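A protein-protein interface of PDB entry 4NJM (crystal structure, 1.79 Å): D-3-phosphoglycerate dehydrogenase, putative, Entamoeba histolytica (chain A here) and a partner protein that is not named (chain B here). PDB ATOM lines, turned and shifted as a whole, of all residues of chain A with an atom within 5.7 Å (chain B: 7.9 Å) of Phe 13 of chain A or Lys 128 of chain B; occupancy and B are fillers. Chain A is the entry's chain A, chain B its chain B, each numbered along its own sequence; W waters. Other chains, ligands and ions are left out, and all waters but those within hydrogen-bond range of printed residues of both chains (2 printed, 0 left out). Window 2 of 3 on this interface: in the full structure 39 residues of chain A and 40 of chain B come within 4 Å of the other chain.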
ATOM      1  N   VAL A   7      -9.464   8.468   5.238  1.00  0.00           N
ATOM      2  CA  VAL A   7      -9.698   7.122   4.744  1.00  0.00           C
ATOM      3  C   VAL A   7      -8.694   6.222   5.433  1.00  0.00           C
ATOM      4  O   VAL A   7      -7.493   6.284   5.161  1.00  0.00           O
ATOM      5  CB  VAL A   7      -9.553   7.033   3.212  1.00  0.00           C
ATOM      6  CG1 VAL A   7      -9.891   5.625   2.730  1.00  0.00           C
ATOM      7  CG2 VAL A   7     -10.448   8.056   2.532  1.00  0.00           C
ATOM      8  N   THR A   9      -7.318   2.727   5.996  1.00  0.00           N
ATOM      9  CA  THR A   9      -7.218   1.405   5.372  1.00  0.00           C
ATOM     10  C   THR A   9      -5.826   0.755   5.528  1.00  0.00           C
ATOM     11  O   THR A   9      -4.906   1.022   4.744  1.00  0.00           O
ATOM     12  CB  THR A   9      -7.575   1.452   3.865  1.00  0.00           C
ATOM     13  OG1 THR A   9      -6.702   2.367   3.189  1.00  0.00           O
ATOM     14  CG2 THR A   9      -9.026   1.873   3.644  1.00  0.00           C
ATOM     15  N   LYS A  11      -5.374  -2.168   4.762  1.00  0.00           N
ATOM     16  CA  LYS A  11      -5.368  -2.881   3.483  1.00  0.00           C
ATOM     17  C   LYS A  11      -5.896  -1.930   2.394  1.00  0.00           C
ATOM     18  O   LYS A  11      -7.110  -1.754   2.255  1.00  0.00           O
ATOM     19  CB  LYS A  11      -6.244  -4.135   3.593  1.00  0.00           C
ATOM     20  CG  LYS A  11      -6.244  -5.040   2.369  1.00  0.00           C
ATOM     21  CD  LYS A  11      -6.990  -6.344   2.644  1.00  0.00           C
ATOM     22  CE  LYS A  11      -8.503  -6.167   2.677  1.00  0.00           C
ATOM     23  NZ  LYS A  11      -9.193  -7.345   3.273  1.00  0.00           N
ATOM     24  N   PRO A  12      -4.984  -1.300   1.628  1.00  0.00           N
ATOM     25  CA  PRO A  12      -5.378  -0.181   0.761  1.00  0.00           C
ATOM     26  C   PRO A  12      -6.286  -0.572  -0.402  1.00  0.00           C
ATOM     27  O   PRO A  12      -6.181  -1.687  -0.922  1.00  0.00           O
ATOM     28  CB  PRO A  12      -4.034   0.331   0.221  1.00  0.00           C
ATOM     29  CG  PRO A  12      -3.026  -0.130   1.225  1.00  0.00           C
ATOM     30  CD  PRO A  12      -3.525  -1.489   1.627  1.00  0.00           C
ATOM     31  N   PHE A  13      -7.181   0.345  -0.773  1.00  0.00           N
ATOM     32  CA  PHE A  13      -8.015   0.209  -1.968  1.00  0.00           C
ATOM     33  C   PHE A  13      -7.143   0.221  -3.217  1.00  0.00           C
ATOM     34  O   PHE A  13      -6.023   0.742  -3.203  1.00  0.00           O
ATOM     35  CB  PHE A  13      -8.989   1.384  -2.090  1.00  0.00           C
ATOM     36  CG  PHE A  13     -10.152   1.343  -1.137  1.00  0.00           C
ATOM     37  CD1 PHE A  13     -11.095   0.322  -1.198  1.00  0.00           C
ATOM     38  CD2 PHE A  13     -10.342   2.374  -0.223  1.00  0.00           C
ATOM     39  CE1 PHE A  13     -12.181   0.303  -0.330  1.00  0.00           C
ATOM     40  CE2 PHE A  13     -11.424   2.365   0.644  1.00  0.00           C
ATOM     41  CZ  PHE A  13     -12.341   1.326   0.594  1.00  0.00           C
ATOM     42  N   ALA A  14      -7.672  -0.341  -4.297  1.00  0.00           N
ATOM     43  CA  ALA A  14      -7.081  -0.202  -5.623  1.00  0.00           C
ATOM     44  C   ALA A  14      -6.908   1.279  -5.953  1.00  0.00           C
ATOM     45  O   ALA A  14      -7.724   2.107  -5.543  1.00  0.00           O
ATOM     46  CB  ALA A  14      -7.974  -0.864  -6.655  1.00  0.00           C
ATOM     47  N   GLU A  15      -5.850   1.602  -6.695  1.00  0.00           N
ATOM     48  CA  GLU A  15      -5.551   2.988  -7.077  1.00  0.00           C
ATOM     49  C   GLU A  15      -6.722   3.705  -7.745  1.00  0.00           C
ATOM     50  O   GLU A  15      -6.974   4.888  -7.470  1.00  0.00           O
ATOM     51  CB  GLU A  15      -4.333   3.042  -7.997  1.00  0.00           C
ATOM     52  CG  GLU A  15      -3.001   2.841  -7.297  1.00  0.00           C
ATOM     53  CD  GLU A  15      -1.841   2.774  -8.272  1.00  0.00           C
ATOM     54  OE1 GLU A  15      -1.823   3.564  -9.241  1.00  0.00           O
ATOM     55  OE2 GLU A  15      -0.945   1.927  -8.068  1.00  0.00           O
ATOM     56  N   ALA A  17      -9.884   3.120  -7.287  1.00  0.00           N
ATOM     57  CA  ALA A  17     -10.896   3.366  -6.266  1.00  0.00           C
ATOM     58  C   ALA A  17     -10.556   4.608  -5.441  1.00  0.00           C
ATOM     59  O   ALA A  17     -11.439   5.425  -5.164  1.00  0.00           O
ATOM     60  CB  ALA A  17     -11.050   2.151  -5.365  1.00  0.00           C
ATOM     61  N   VAL A  18      -9.282   4.744  -5.066  1.00  0.00           N
ATOM     62  CA  VAL A  18      -8.795   5.912  -4.317  1.00  0.00           C
ATOM     63  C   VAL A  18      -8.963   7.190  -5.145  1.00  0.00           C
ATOM     64  O   VAL A  18      -9.354   8.235  -4.608  1.00  0.00           O
ATOM     65  CB  VAL A  18      -7.324   5.752  -3.866  1.00  0.00           C
ATOM     66  CG1 VAL A  18      -6.776   7.058  -3.296  1.00  0.00           C
ATOM     67  CG2 VAL A  18      -7.191   4.648  -2.829  1.00  0.00           C
ATOM     68  N   ILE A  21     -12.584   8.041  -5.052  1.00  0.00           N
ATOM     69  CA  ILE A  21     -12.909   8.647  -3.753  1.00  0.00           C
ATOM     70  C   ILE A  21     -12.543  10.130  -3.754  1.00  0.00           C
ATOM     71  O   ILE A  21     -13.360  10.977  -3.379  1.00  0.00           O
ATOM     72  CB  ILE A  21     -12.224   7.912  -2.575  1.00  0.00           C
ATOM     73  CG1 ILE A  21     -12.876   6.538  -2.355  1.00  0.00           C
ATOM     74  CG2 ILE A  21     -12.308   8.730  -1.293  1.00  0.00           C
ATOM     75  CD1 ILE A  21     -12.013   5.546  -1.597  1.00  0.00           C
ATOM     76  N   MET A  34      -5.427  10.319   3.292  1.00  0.00           N
ATOM     77  CA  MET A  34      -5.274   8.864   3.250  1.00  0.00           C
ATOM     78  C   MET A  34      -4.383   8.380   4.387  1.00  0.00           C
ATOM     79  O   MET A  34      -3.289   8.908   4.585  1.00  0.00           O
ATOM     80  CB  MET A  34      -4.679   8.408   1.911  1.00  0.00           C
ATOM     81  CG  MET A  34      -5.479   8.801   0.677  1.00  0.00           C
ATOM     82  SD  MET A  34      -7.175   8.195   0.648  1.00  0.00           S
ATOM     83  CE  MET A  34      -6.899   6.424   0.524  1.00  0.00           C
ATOM     84  N   GLU A  36      -2.936   4.948   4.935  1.00  0.00           N
ATOM     85  CA  GLU A  36      -2.821   3.654   4.266  1.00  0.00           C
ATOM     86  C   GLU A  36      -1.666   2.808   4.778  1.00  0.00           C
ATOM     87  O   GLU A  36      -0.566   3.317   5.028  1.00  0.00           O
ATOM     88  CB  GLU A  36      -2.676   3.844   2.759  1.00  0.00           C
ATOM     89  CG  GLU A  36      -3.929   4.363   2.074  1.00  0.00           C
ATOM     90  CD  GLU A  36      -3.718   4.601   0.594  1.00  0.00           C
ATOM     91  OE1 GLU A  36      -2.820   5.388   0.231  1.00  0.00           O
ATOM     92  OE2 GLU A  36      -4.462   4.008  -0.211  1.00  0.00           O
ATOM     93  N   ILE A  55     -13.828   7.075   6.363  1.00  0.00           N
ATOM     94  CA  ILE A  55     -14.101   5.910   5.518  1.00  0.00           C
ATOM     95  C   ILE A  55     -13.141   4.814   5.969  1.00  0.00           C
ATOM     96  O   ILE A  55     -11.941   5.042   6.079  1.00  0.00           O
ATOM     97  CB  ILE A  55     -13.884   6.201   4.014  1.00  0.00           C
ATOM     98  CG1 ILE A  55     -14.851   7.287   3.524  1.00  0.00           C
ATOM     99  CG2 ILE A  55     -14.057   4.922   3.193  1.00  0.00           C
ATOM    100  CD1 ILE A  55     -14.571   7.770   2.116  1.00  0.00           C
ATOM    101  N   VAL A  56     -13.675   3.630   6.244  1.00  0.00           N
ATOM    102  CA  VAL A  56     -12.877   2.536   6.789  1.00  0.00           C
ATOM    103  C   VAL A  56     -13.241   1.221   6.090  1.00  0.00           C
ATOM    104  O   VAL A  56     -14.331   1.086   5.532  1.00  0.00           O
ATOM    105  CB  VAL A  56     -13.061   2.437   8.329  1.00  0.00           C
ATOM    106  CG1 VAL A  56     -14.472   1.984   8.683  1.00  0.00           C
ATOM    107  CG2 VAL A  56     -12.024   1.511   8.950  1.00  0.00           C
ATOM    108  N   ARG A  57     -12.310   0.274   6.085  1.00  0.00           N
ATOM    109  CA  ARG A  57     -12.617  -1.077   5.644  1.00  0.00           C
ATOM    110  C   ARG A  57     -12.777  -1.969   6.867  1.00  0.00           C
ATOM    111  O   ARG A  57     -13.620  -1.678   7.722  1.00  0.00           O
ATOM    112  CB  ARG A  57     -11.568  -1.598   4.665  1.00  0.00           C
ATOM    113  CG  ARG A  57     -11.851  -1.158   3.247  1.00  0.00           C
ATOM    114  CD  ARG A  57     -11.737  -2.340   2.298  1.00  0.00           C
ATOM    115  NE  ARG A  57     -10.443  -2.323   1.677  1.00  0.00           N
ATOM    116  CZ  ARG A  57      -9.976  -3.201   0.800  1.00  0.00           C
ATOM    117  NH1 ARG A  57     -10.681  -4.266   0.404  1.00  0.00           N
ATOM    118  NH2 ARG A  57      -8.766  -2.992   0.322  1.00  0.00           N
ATOM    119  N   ALA A  78     -16.773   1.082   3.992  1.00  0.00           N
ATOM    120  CA  ALA A  78     -16.858   0.730   2.581  1.00  0.00           C
ATOM    121  C   ALA A  78     -16.870  -0.788   2.509  1.00  0.00           C
ATOM    122  O   ALA A  78     -15.819  -1.429   2.567  1.00  0.00           O
ATOM    123  CB  ALA A  78     -15.671   1.299   1.828  1.00  0.00           C
ATOM    124  N   GLU A 269     -10.996  -8.011  -2.489  1.00  0.00           N
ATOM    125  CA  GLU A 269      -9.752  -7.491  -3.055  1.00  0.00           C
ATOM    126  C   GLU A 269      -9.756  -7.617  -4.575  1.00  0.00           C
ATOM    127  O   GLU A 269      -8.979  -8.378  -5.153  1.00  0.00           O
ATOM    128  CB  GLU A 269      -8.535  -8.199  -2.456  1.00  0.00           C
ATOM    129  CG  GLU A 269      -8.149  -7.711  -1.067  1.00  0.00           C
ATOM    130  CD  GLU A 269      -7.629  -6.287  -1.105  1.00  0.00           C
ATOM    131  OE1 GLU A 269      -6.395  -6.116  -1.143  1.00  0.00           O
ATOM    132  OE2 GLU A 269      -8.448  -5.348  -1.134  1.00  0.00           O
ATOM    133  N   THR A 270     -10.659  -6.886  -5.213  1.00  0.00           N
ATOM    134  CA  THR A 270     -10.682  -6.813  -6.673  1.00  0.00           C
ATOM    135  C   THR A 270     -10.806  -5.362  -7.074  1.00  0.00           C
ATOM    136  O   THR A 270     -11.308  -4.548  -6.307  1.00  0.00           O
ATOM    137  CB  THR A 270     -11.871  -7.580  -7.281  1.00  0.00           C
ATOM    138  OG1 THR A 270     -13.096  -6.964  -6.875  1.00  0.00           O
ATOM    139  CG2 THR A 270     -11.869  -9.053  -6.837  1.00  0.00           C
ATOM    140  N   GLU A 271     -10.361  -5.055  -8.286  1.00  0.00           N
ATOM    141  CA  GLU A 271     -10.530  -3.740  -8.885  1.00  0.00           C
ATOM    142  C   GLU A 271     -11.989  -3.285  -8.815  1.00  0.00           C
ATOM    143  O   GLU A 271     -12.277  -2.167  -8.369  1.00  0.00           O
ATOM    144  CB  GLU A 271     -10.056  -3.789 -10.348  1.00  0.00           C
ATOM    145  CG  GLU A 271     -10.340  -2.539 -11.174  1.00  0.00           C
ATOM    146  CD  GLU A 271      -9.277  -1.467 -11.023  1.00  0.00           C
ATOM    147  OE1 GLU A 271      -9.348  -0.461 -11.766  1.00  0.00           O
ATOM    148  OE2 GLU A 271      -8.366  -1.623 -10.176  1.00  0.00           O
ATOM    149  N   ASN A 274     -13.563  -2.862  -5.127  1.00  0.00           N
ATOM    150  CA  ASN A 274     -12.948  -1.668  -4.510  1.00  0.00           C
ATOM    151  C   ASN A 274     -13.546  -0.366  -5.048  1.00  0.00           C
ATOM    152  O   ASN A 274     -13.882   0.545  -4.279  1.00  0.00           O
ATOM    153  CB  ASN A 274     -11.436  -1.648  -4.719  1.00  0.00           C
ATOM    154  CG  ASN A 274     -10.684  -2.570  -3.777  1.00  0.00           C
ATOM    155  OD1 ASN A 274     -11.264  -3.303  -2.955  1.00  0.00           O
ATOM    156  ND2 ASN A 274      -9.376  -2.543  -3.895  1.00  0.00           N
ATOM    157  N   ALA A 277     -17.312  -0.122  -3.652  1.00  0.00           N
ATOM    158  CA  ALA A 277     -17.437   0.175  -2.222  1.00  0.00           C
ATOM    159  C   ALA A 277     -16.836   1.534  -1.879  1.00  0.00           C
ATOM    160  O   ALA A 277     -17.454   2.320  -1.153  1.00  0.00           O
ATOM    161  CB  ALA A 277     -16.813  -0.931  -1.382  1.00  0.00           C
ATOM    162  N   GLY A 278     -15.644   1.806  -2.407  1.00  0.00           N
ATOM    163  CA  GLY A 278     -14.928   3.046  -2.114  1.00  0.00           C
ATOM    164  C   GLY A 278     -15.722   4.259  -2.554  1.00  0.00           C
ATOM    165  O   GLY A 278     -15.890   5.220  -1.794  1.00  0.00           O
ATOM    166  N   GLY B 119      -7.119 -18.077 -11.415  1.00  0.00           N
ATOM    167  CA  GLY B 119      -6.238 -17.250 -12.229  1.00  0.00           C
ATOM    168  C   GLY B 119      -6.470 -15.758 -12.069  1.00  0.00           C
ATOM    169  O   GLY B 119      -5.511 -14.988 -11.980  1.00  0.00           O
ATOM    170  N   PHE B 120      -7.736 -15.349 -12.034  1.00  0.00           N
ATOM    171  CA  PHE B 120      -8.111 -13.942 -11.845  1.00  0.00           C
ATOM    172  C   PHE B 120      -7.926 -13.435 -10.408  1.00  0.00           C
ATOM    173  O   PHE B 120      -7.942 -12.226 -10.168  1.00  0.00           O
ATOM    174  CB  PHE B 120      -9.570 -13.735 -12.279  1.00  0.00           C
ATOM    175  CG  PHE B 120      -9.732 -12.984 -13.590  1.00  0.00           C
ATOM    176  CD1 PHE B 120      -8.747 -13.019 -14.572  1.00  0.00           C
ATOM    177  CD2 PHE B 120     -10.894 -12.246 -13.833  1.00  0.00           C
ATOM    178  CE1 PHE B 120      -8.920 -12.337 -15.781  1.00  0.00           C
ATOM    179  CE2 PHE B 120     -11.068 -11.556 -15.025  1.00  0.00           C
ATOM    180  CZ  PHE B 120     -10.078 -11.601 -15.999  1.00  0.00           C
ATOM    181  N   ARG B 121      -7.767 -14.354  -9.466  1.00  0.00           N
ATOM    182  CA  ARG B 121      -7.701 -13.995  -8.045  1.00  0.00           C
ATOM    183  C   ARG B 121      -6.350 -14.370  -7.444  1.00  0.00           C
ATOM    184  O   ARG B 121      -6.261 -14.822  -6.292  1.00  0.00           O
ATOM    185  CB  ARG B 121      -8.864 -14.626  -7.269  1.00  0.00           C
ATOM    186  CG  ARG B 121     -10.240 -14.205  -7.777  1.00  0.00           C
ATOM    187  CD  ARG B 121     -10.468 -12.705  -7.606  1.00  0.00           C
ATOM    188  NE  ARG B 121     -10.786 -12.355  -6.219  1.00  0.00           N
ATOM    189  CZ  ARG B 121     -12.023 -12.317  -5.716  1.00  0.00           C
ATOM    190  NH1 ARG B 121     -13.084 -12.617  -6.475  1.00  0.00           N
ATOM    191  NH2 ARG B 121     -12.207 -11.994  -4.446  1.00  0.00           N
ATOM    192  N   LYS B 122      -5.306 -14.173  -8.249  1.00  0.00           N
ATOM    193  CA  LYS B 122      -3.903 -14.299  -7.817  1.00  0.00           C
ATOM    194  C   LYS B 122      -3.582 -15.656  -7.197  1.00  0.00           C
ATOM    195  O   LYS B 122      -2.750 -15.751  -6.294  1.00  0.00           O
ATOM    196  CB  LYS B 122      -3.527 -13.194  -6.818  1.00  0.00           C
ATOM    197  CG  LYS B 122      -3.933 -11.782  -7.210  1.00  0.00           C
ATOM    198  CD  LYS B 122      -3.025 -11.189  -8.268  1.00  0.00           C
ATOM    199  CE  LYS B 122      -1.735 -10.658  -7.677  1.00  0.00           C
ATOM    200  NZ  LYS B 122      -0.925 -10.072  -8.775  1.00  0.00           N
ATOM    201  N   LYS B 125      -3.779 -15.941  -3.373  1.00  0.00           N
ATOM    202  CA  LYS B 125      -2.774 -15.238  -2.584  1.00  0.00           C
ATOM    203  C   LYS B 125      -3.201 -13.779  -2.447  1.00  0.00           C
ATOM    204  O   LYS B 125      -4.222 -13.361  -3.004  1.00  0.00           O
ATOM    205  CB  LYS B 125      -1.411 -15.313  -3.281  1.00  0.00           C
ATOM    206  CG  LYS B 125      -0.830 -16.715  -3.374  1.00  0.00           C
ATOM    207  CD  LYS B 125       0.610 -16.655  -3.850  1.00  0.00           C
ATOM    208  CE  LYS B 125       1.290 -18.008  -3.740  1.00  0.00           C
ATOM    209  NZ  LYS B 125       0.910 -18.904  -4.861  1.00  0.00           N
ATOM    210  N   GLU B 126      -2.397 -13.014  -1.715  1.00  0.00           N
ATOM    211  CA  GLU B 126      -2.618 -11.590  -1.487  1.00  0.00           C
ATOM    212  C   GLU B 126      -2.543 -10.789  -2.790  1.00  0.00           C
ATOM    213  O   GLU B 126      -1.884 -11.204  -3.747  1.00  0.00           O
ATOM    214  CB  GLU B 126      -1.545 -11.103  -0.516  1.00  0.00           C
ATOM    215  CG  GLU B 126      -1.768  -9.742   0.107  1.00  0.00           C
ATOM    216  CD  GLU B 126      -0.654  -9.382   1.072  1.00  0.00           C
ATOM    217  OE1 GLU B 126       0.456  -9.933   0.925  1.00  0.00           O
ATOM    218  OE2 GLU B 126      -0.882  -8.555   1.975  1.00  0.00           O
ATOM    219  N   GLY B 127      -3.211  -9.641  -2.828  1.00  0.00           N
ATOM    220  CA  GLY B 127      -3.118  -8.751  -3.979  1.00  0.00           C
ATOM    221  C   GLY B 127      -4.455  -8.429  -4.614  1.00  0.00           C
ATOM    222  O   GLY B 127      -5.492  -8.964  -4.216  1.00  0.00           O
ATOM    223  N   LYS B 128      -4.428  -7.544  -5.605  1.00  0.00           N
ATOM    224  CA  LYS B 128      -5.655  -7.091  -6.245  1.00  0.00           C
ATOM    225  C   LYS B 128      -6.015  -7.997  -7.407  1.00  0.00           C
ATOM    226  O   LYS B 128      -5.246  -8.128  -8.355  1.00  0.00           O
ATOM    227  CB  LYS B 128      -5.521  -5.636  -6.715  1.00  0.00           C
ATOM    228  CG  LYS B 128      -5.387  -4.633  -5.576  1.00  0.00           C
ATOM    229  CD  LYS B 128      -6.664  -4.569  -4.751  1.00  0.00           C
ATOM    230  CE  LYS B 128      -6.611  -3.447  -3.729  1.00  0.00           C
ATOM    231  NZ  LYS B 128      -5.844  -3.782  -2.503  1.00  0.00           N
ATOM    232  N   GLY B 129      -7.183  -8.624  -7.323  1.00  0.00           N
ATOM    233  CA  GLY B 129      -7.655  -9.493  -8.402  1.00  0.00           C
ATOM    234  C   GLY B 129      -8.695  -8.828  -9.281  1.00  0.00           C
ATOM    235  O   GLY B 129      -8.909  -7.623  -9.203  1.00  0.00           O
ATOM    236  N   ARG B 130      -9.339  -9.632 -10.121  1.00  0.00           N
ATOM    237  CA  ARG B 130     -10.412  -9.165 -10.983  1.00  0.00           C
ATOM    238  C   ARG B 130     -11.567 -10.154 -10.962  1.00  0.00           C
ATOM    239  O   ARG B 130     -11.413 -11.293 -10.508  1.00  0.00           O
ATOM    240  CB  ARG B 130      -9.897  -9.003 -12.418  1.00  0.00           C
ATOM    241  CG  ARG B 130      -9.013  -7.786 -12.612  1.00  0.00           C
ATOM    242  CD  ARG B 130      -8.359  -7.829 -13.977  1.00  0.00           C
ATOM    243  NE  ARG B 130      -7.285  -8.814 -13.989  1.00  0.00           N
ATOM    244  CZ  ARG B 130      -6.830  -9.407 -15.087  1.00  0.00           C
ATOM    245  NH1 ARG B 130      -7.366  -9.121 -16.266  1.00  0.00           N
ATOM    246  NH2 ARG B 130      -5.847 -10.284 -15.000  1.00  0.00           N
HETATM  247  O   HOH W   1      -4.767  -8.359  -0.638  1.00  0.00           O
HETATM  248  O   HOH W   2      -8.551 -11.160  -5.296  1.00  0.00           O
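O of Glu 269 of chain A sits at hydrogen-bond distance from N of Gly 129 of chain B (2.8 Å).
The backbone NH (N) of Glu 271 of chain A lies within hydrogen-bond range of the backbone carbonyl oxygen (O) of Gly 129 of chain B (3.1 Å).
The side-chain carboxylate of Glu 269 of chain A is in salt-bridge range of the side-chain amino group of Lys 128 of chain B (2.8 Å).
The backbone carbonyl oxygen (O) of Pro 12 of chain A lies within hydrogen-bond range of the side-chain amino group (NZ) of Lys 128 of chain B, at 2.6 Å.
The backbone NH (N) of Ala 14 of chain A lies close to the side-chain amide nitrogen (ND2) of Asn 274 of chain A (2.8 Å).
O of Pro 12 of chain A sits at hydrogen-bond distance from NH2 of Arg 57 of chain A (3.2 Å).
The guanidinium group (NH2) of Arg 57 of chain A is in salt-bridge range of the side-chain carboxylate (OE2) of Glu 269 of chain A (2.8 Å).
Phe 13 of chain A touches Lys 128 of chain B (C to CE, 3.7 Å).
Lys 128 of chain B touches Ala 14 of chain A (CE to N, 3.3 Å).
Gly 127 of chain B touches Glu 269 of chain A.
Arg 121 of chain B touches Thr 270 of chain A (CZ to CG2, 3.5 Å).
Thr 270 of chain A touches Gly 129 of chain B (CA to O, 3.2 Å).
Asn 274 of chain A touches Lys 128 of chain B.
Phe 13 of chain A touches just one residue of chain B: Lys 128 (3.7 Å).
Ala 14 of chain A touches one residue of chain B.
Printed residues of chain B within 4 Å of Glu 269 of chain A: Gly 127, Lys 128 and Gly 129.
Of chain A, only Pro 12, Phe 13, Ala 14, Glu 269 and Asn 274 come within 4 Å of Lys 128 of chain B.
Of the printed residues of chain A, Gly 129 of chain B touches Glu 269 (2.8 Å), Thr 270 (3.2 Å) and Glu 271 (3.1 Å).
The nearest printed residue of chain B that does not touch Phe 13 of chain A is Gly 127 of chain B (9.2 Å).
The nearest residue of chain A that does not touch Lys 128 of chain B is Arg 57 of chain A (4.1 Å).
Of the 10 printed residues of chain B, 4 touch a printed residue of chain A.
Among the printed residues, Asp or Glu carboxylates within 4 Å of a Lys or Arg side-chain nitrogen of the other chain: Glu 269 of chain A with Lys 128 of chain B (2.8 Å).
Water W2 bridges NE of Arg 121 of chain B (2.7 Å) and O of Glu 269 of chain A (2.8 Å).
Water W1 bridges OE1 of Glu 269 of chain A (2.8 Å) and N of Gly 127 of chain B (3.0 Å).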
